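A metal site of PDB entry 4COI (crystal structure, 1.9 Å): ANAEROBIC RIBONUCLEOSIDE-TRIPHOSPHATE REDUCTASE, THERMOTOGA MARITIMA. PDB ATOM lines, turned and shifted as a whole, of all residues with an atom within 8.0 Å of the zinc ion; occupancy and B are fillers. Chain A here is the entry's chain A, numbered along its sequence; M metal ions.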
ATOM      1  N   GLU A 276      -1.978   1.424   2.679  1.00  0.00           N
ATOM      2  CA  GLU A 276      -1.570   0.801   1.421  1.00  0.00           C
ATOM      3  C   GLU A 276      -2.596   1.051   0.334  1.00  0.00           C
ATOM      4  O   GLU A 276      -2.247   1.194  -0.837  1.00  0.00           O
ATOM      5  CB  GLU A 276      -1.398  -0.717   1.569  1.00  0.00           C
ATOM      6  CG  GLU A 276      -0.459  -1.164   2.670  1.00  0.00           C
ATOM      7  CD  GLU A 276      -0.159  -2.654   2.591  1.00  0.00           C
ATOM      8  OE1 GLU A 276       0.292  -3.129   1.532  1.00  0.00           O
ATOM      9  OE2 GLU A 276      -0.381  -3.365   3.604  1.00  0.00           O
ATOM     10  N   ARG A 277      -3.868   1.073   0.732  1.00  0.00           N
ATOM     11  CA  ARG A 277      -4.962   1.305  -0.190  1.00  0.00           C
ATOM     12  C   ARG A 277      -5.061   2.792  -0.511  1.00  0.00           C
ATOM     13  O   ARG A 277      -5.359   3.181  -1.639  1.00  0.00           O
ATOM     14  CB  ARG A 277      -6.287   0.816   0.408  1.00  0.00           C
ATOM     15  CG  ARG A 277      -6.257  -0.645   0.866  1.00  0.00           C
ATOM     16  CD  ARG A 277      -7.665  -1.183   1.115  1.00  0.00           C
ATOM     17  NE  ARG A 277      -7.667  -2.559   1.585  1.00  0.00           N
ATOM     18  CZ  ARG A 277      -7.615  -3.630   0.803  1.00  0.00           C
ATOM     19  NH1 ARG A 277      -7.546  -3.496  -0.521  1.00  0.00           N
ATOM     20  NH2 ARG A 277      -7.624  -4.848   1.327  1.00  0.00           N
ATOM     21  N   GLN A 278      -4.810   3.622   0.499  1.00  0.00           N
ATOM     22  CA  GLN A 278      -4.899   5.069   0.352  1.00  0.00           C
ATOM     23  C   GLN A 278      -4.278   5.791   1.549  1.00  0.00           C
ATOM     24  O   GLN A 278      -4.672   5.584   2.700  1.00  0.00           O
ATOM     25  CB  GLN A 278      -6.362   5.485   0.187  1.00  0.00           C
ATOM     26  CG  GLN A 278      -6.554   6.906  -0.307  1.00  0.00           C
ATOM     27  CD  GLN A 278      -5.995   7.149  -1.709  1.00  0.00           C
ATOM     28  OE1 GLN A 278      -5.796   8.292  -2.107  1.00  0.00           O
ATOM     29  NE2 GLN A 278      -5.725   6.072  -2.446  1.00  0.00           N
ATOM     30  N   VAL A 593       4.009   8.182  -2.156  1.00  0.00           N
ATOM     31  CA  VAL A 593       2.685   7.954  -2.735  1.00  0.00           C
ATOM     32  C   VAL A 593       2.750   8.022  -4.248  1.00  0.00           C
ATOM     33  O   VAL A 593       3.560   8.762  -4.796  1.00  0.00           O
ATOM     34  CB  VAL A 593       1.646   8.985  -2.260  1.00  0.00           C
ATOM     35  CG1 VAL A 593       1.259   8.740  -0.813  1.00  0.00           C
ATOM     36  CG2 VAL A 593       2.161  10.397  -2.447  1.00  0.00           C
ATOM     37  N   CYS A 594       1.901   7.231  -4.895  1.00  0.00           N
ATOM     38  CA  CYS A 594       1.723   7.296  -6.335  1.00  0.00           C
ATOM     39  C   CYS A 594       0.559   8.235  -6.650  1.00  0.00           C
ATOM     40  O   CYS A 594      -0.049   8.820  -5.753  1.00  0.00           O
ATOM     41  CB  CYS A 594       1.431   5.903  -6.909  1.00  0.00           C
ATOM     42  SG  CYS A 594      -0.157   5.201  -6.423  1.00  0.00           S
ATOM     43  N   GLU A 595       0.254   8.366  -7.935  1.00  0.00           N
ATOM     44  CA  GLU A 595      -0.789   9.286  -8.383  1.00  0.00           C
ATOM     45  C   GLU A 595      -2.179   8.809  -7.958  1.00  0.00           C
ATOM     46  O   GLU A 595      -3.121   9.598  -7.913  1.00  0.00           O
ATOM     47  CB  GLU A 595      -0.729   9.461  -9.894  1.00  0.00           C
ATOM     48  CG  GLU A 595      -1.024   8.207 -10.695  1.00  0.00           C
ATOM     49  CD  GLU A 595      -0.839   8.400 -12.182  1.00  0.00           C
ATOM     50  OE1 GLU A 595      -0.294   9.451 -12.585  1.00  0.00           O
ATOM     51  OE2 GLU A 595      -1.228   7.496 -12.946  1.00  0.00           O
ATOM     52  N   ASP A 596      -2.297   7.528  -7.636  1.00  0.00           N
ATOM     53  CA  ASP A 596      -3.573   6.951  -7.214  1.00  0.00           C
ATOM     54  C   ASP A 596      -3.675   6.832  -5.689  1.00  0.00           C
ATOM     55  O   ASP A 596      -4.666   6.306  -5.166  1.00  0.00           O
ATOM     56  CB  ASP A 596      -3.804   5.600  -7.885  1.00  0.00           C
ATOM     57  CG  ASP A 596      -3.995   5.719  -9.382  1.00  0.00           C
ATOM     58  OD1 ASP A 596      -4.448   6.793  -9.846  1.00  0.00           O
ATOM     59  OD2 ASP A 596      -3.699   4.744 -10.115  1.00  0.00           O
ATOM     60  N   GLY A 597      -2.655   7.302  -4.979  1.00  0.00           N
ATOM     61  CA  GLY A 597      -2.765   7.520  -3.543  1.00  0.00           C
ATOM     62  C   GLY A 597      -2.319   6.387  -2.637  1.00  0.00           C
ATOM     63  O   GLY A 597      -2.467   6.482  -1.416  1.00  0.00           O
ATOM     64  N   HIS A 598      -1.747   5.328  -3.205  1.00  0.00           N
ATOM     65  CA  HIS A 598      -1.262   4.214  -2.394  1.00  0.00           C
ATOM     66  C   HIS A 598      -0.010   4.646  -1.628  1.00  0.00           C
ATOM     67  O   HIS A 598       0.776   5.427  -2.141  1.00  0.00           O
ATOM     68  CB  HIS A 598      -0.936   3.017  -3.277  1.00  0.00           C
ATOM     69  CG  HIS A 598      -2.019   2.669  -4.250  1.00  0.00           C
ATOM     70  ND1 HIS A 598      -1.796   2.617  -5.610  1.00  0.00           N
ATOM     71  CD2 HIS A 598      -3.322   2.364  -4.065  1.00  0.00           C
ATOM     72  CE1 HIS A 598      -2.916   2.291  -6.223  1.00  0.00           C
ATOM     73  NE2 HIS A 598      -3.863   2.131  -5.308  1.00  0.00           N
ATOM     74  N   ALA A 599       0.157   4.162  -0.407  1.00  0.00           N
ATOM     75  CA  ALA A 599       1.337   4.464   0.391  1.00  0.00           C
ATOM     76  C   ALA A 599       2.304   3.288   0.341  1.00  0.00           C
ATOM     77  O   ALA A 599       1.880   2.136   0.360  1.00  0.00           O
ATOM     78  CB  ALA A 599       0.960   4.741   1.831  1.00  0.00           C
ATOM     79  N   PHE A 600       3.596   3.608   0.294  1.00  0.00           N
ATOM     80  CA  PHE A 600       4.659   2.603   0.219  1.00  0.00           C
ATOM     81  C   PHE A 600       6.028   3.259   0.383  1.00  0.00           C
ATOM     82  O   PHE A 600       6.142   4.458   0.678  1.00  0.00           O
ATOM     83  CB  PHE A 600       4.593   1.882  -1.115  1.00  0.00           C
ATOM     84  CG  PHE A 600       4.809   2.780  -2.291  1.00  0.00           C
ATOM     85  CD1 PHE A 600       6.081   3.052  -2.755  1.00  0.00           C
ATOM     86  CD2 PHE A 600       3.727   3.372  -2.930  1.00  0.00           C
ATOM     87  CE1 PHE A 600       6.278   3.882  -3.829  1.00  0.00           C
ATOM     88  CE2 PHE A 600       3.924   4.203  -4.004  1.00  0.00           C
ATOM     89  CZ  PHE A 600       5.203   4.457  -4.457  1.00  0.00           C
ATOM     90  N   ARG A 604       8.722   2.788  -6.811  1.00  0.00           N
ATOM     91  CA  ARG A 604       7.672   2.109  -7.564  1.00  0.00           C
ATOM     92  C   ARG A 604       6.597   1.563  -6.625  1.00  0.00           C
ATOM     93  O   ARG A 604       6.898   1.010  -5.567  1.00  0.00           O
ATOM     94  CB  ARG A 604       8.263   0.975  -8.409  1.00  0.00           C
ATOM     95  CG  ARG A 604       7.239   0.218  -9.252  1.00  0.00           C
ATOM     96  CD  ARG A 604       7.911  -0.779 -10.206  1.00  0.00           C
ATOM     97  NE  ARG A 604       6.938  -1.660 -10.867  1.00  0.00           N
ATOM     98  CZ  ARG A 604       6.557  -1.578 -12.150  1.00  0.00           C
ATOM     99  NH1 ARG A 604       7.058  -0.647 -12.955  1.00  0.00           N
ATOM    100  NH2 ARG A 604       5.675  -2.442 -12.624  1.00  0.00           N
ATOM    101  N   CYS A 605       5.331   1.711  -7.024  1.00  0.00           N
ATOM    102  CA  CYS A 605       4.201   1.292  -6.218  1.00  0.00           C
ATOM    103  C   CYS A 605       4.031  -0.226  -6.267  1.00  0.00           C
ATOM    104  O   CYS A 605       3.923  -0.797  -7.342  1.00  0.00           O
ATOM    105  CB  CYS A 605       2.920   1.979  -6.694  1.00  0.00           C
ATOM    106  SG  CYS A 605       1.454   1.724  -5.620  1.00  0.00           S
ATOM    107  N   PRO A 606       4.015  -0.886  -5.099  1.00  0.00           N
ATOM    108  CA  PRO A 606       3.803  -2.338  -5.126  1.00  0.00           C
ATOM    109  C   PRO A 606       2.382  -2.692  -5.543  1.00  0.00           C
ATOM    110  O   PRO A 606       2.134  -3.797  -6.046  1.00  0.00           O
ATOM    111  CB  PRO A 606       4.041  -2.743  -3.673  1.00  0.00           C
ATOM    112  CG  PRO A 606       3.663  -1.543  -2.893  1.00  0.00           C
ATOM    113  CD  PRO A 606       4.157  -0.393  -3.720  1.00  0.00           C
ATOM    114  N   VAL A 607       1.452  -1.763  -5.352  1.00  0.00           N
ATOM    115  CA  VAL A 607       0.048  -2.010  -5.651  1.00  0.00           C
ATOM    116  C   VAL A 607      -0.243  -1.882  -7.144  1.00  0.00           C
ATOM    117  O   VAL A 607      -0.785  -2.810  -7.747  1.00  0.00           O
ATOM    118  CB  VAL A 607      -0.867  -1.041  -4.864  1.00  0.00           C
ATOM    119  CG1 VAL A 607      -2.332  -1.325  -5.151  1.00  0.00           C
ATOM    120  CG2 VAL A 607      -0.600  -1.168  -3.365  1.00  0.00           C
ATOM    121  N   CYS A 608       0.128  -0.752  -7.743  1.00  0.00           N
ATOM    122  CA  CYS A 608      -0.256  -0.451  -9.127  1.00  0.00           C
ATOM    123  C   CYS A 608       0.928  -0.257 -10.075  1.00  0.00           C
ATOM    124  O   CYS A 608       0.746  -0.016 -11.272  1.00  0.00           O
ATOM    125  CB  CYS A 608      -1.154   0.796  -9.162  1.00  0.00           C
ATOM    126  SG  CYS A 608      -0.290   2.348  -8.928  1.00  0.00           S
ATOM    127  N   GLY A 609       2.147  -0.369  -9.551  1.00  0.00           N
ATOM    128  CA  GLY A 609       3.338  -0.342 -10.382  1.00  0.00           C
ATOM    129  C   GLY A 609       3.762   1.041 -10.808  1.00  0.00           C
ATOM    130  O   GLY A 609       4.835   1.213 -11.378  1.00  0.00           O
ATOM    131  N   LYS A 610       2.925   2.042 -10.543  1.00  0.00           N
ATOM    132  CA  LYS A 610       3.212   3.401 -10.987  1.00  0.00           C
ATOM    133  C   LYS A 610       4.291   4.069 -10.148  1.00  0.00           C
ATOM    134  O   LYS A 610       4.706   3.561  -9.113  1.00  0.00           O
ATOM    135  CB  LYS A 610       1.940   4.241 -10.951  1.00  0.00           C
ATOM    136  CG  LYS A 610       0.878   3.770 -11.893  1.00  0.00           C
ATOM    137  CD  LYS A 610      -0.150   4.841 -12.085  1.00  0.00           C
ATOM    138  CE  LYS A 610      -1.360   4.323 -12.827  1.00  0.00           C
ATOM    139  NZ  LYS A 610      -2.508   5.240 -12.650  1.00  0.00           N
ATOM    140  N   ALA A 611       4.731   5.240 -10.616  1.00  0.00           N
ATOM    141  CA  ALA A 611       5.840   5.933  -9.993  1.00  0.00           C
ATOM    142  C   ALA A 611       5.398   6.789  -8.814  1.00  0.00           C
ATOM    143  O   ALA A 611       4.322   7.373  -8.823  1.00  0.00           O
ATOM    144  CB  ALA A 611       6.554   6.796 -11.014  1.00  0.00           C
ATOM    145  N   LYS A 612       6.256   6.823  -7.789  1.00  0.00           N
ATOM    146  CA  LYS A 612       6.193   7.811  -6.726  1.00  0.00           C
ATOM    147  C   LYS A 612       6.056   9.207  -7.315  1.00  0.00           C
ATOM    148  O   LYS A 612       6.782   9.567  -8.245  1.00  0.00           O
ATOM    149  CB  LYS A 612       7.466   7.715  -5.895  1.00  0.00           C
ATOM    150  CG  LYS A 612       7.914   9.020  -5.263  1.00  0.00           C
ATOM    151  CD  LYS A 612       9.063   8.780  -4.290  1.00  0.00           C
ATOM    152  CE  LYS A 612       9.358  10.034  -3.488  1.00  0.00           C
ATOM    153  NZ  LYS A 612      10.386   9.791  -2.442  1.00  0.00           N
HETATM  154 ZN    ZN M   1      -0.154   2.943  -6.729  1.00  0.00          ZN
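SG of Cys 594 sits close to N of Asp 596.
SG of Cys 594 lies close to N of Gly 597 (3.6 Å).
The side-chain sulfur (SG) of Cys 608 sits close to the backbone NH (N) of Lys 610 (3.6 Å).
SG of Cys 605 sits close to N of Val 607 (3.5 Å).
The backbone NH (N) of Cys 605 sits at hydrogen-bond distance from the backbone carbonyl oxygen (O) of Lys 610, 2.9 Å away.
Of the 20 residues printed, 4 come within 4 Å of the zinc ion.
The zinc ion is bound by a ring nitrogen (ND1) of His 598 (2.0 Å), the side-chain sulfur of Cys 594 (2.3 Å), the side-chain sulfur of Cys 608 (2.3 Å) and the side-chain sulfur of Cys 605 (2.3 Å).
The zinc ion has four donor atoms within binding distance.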
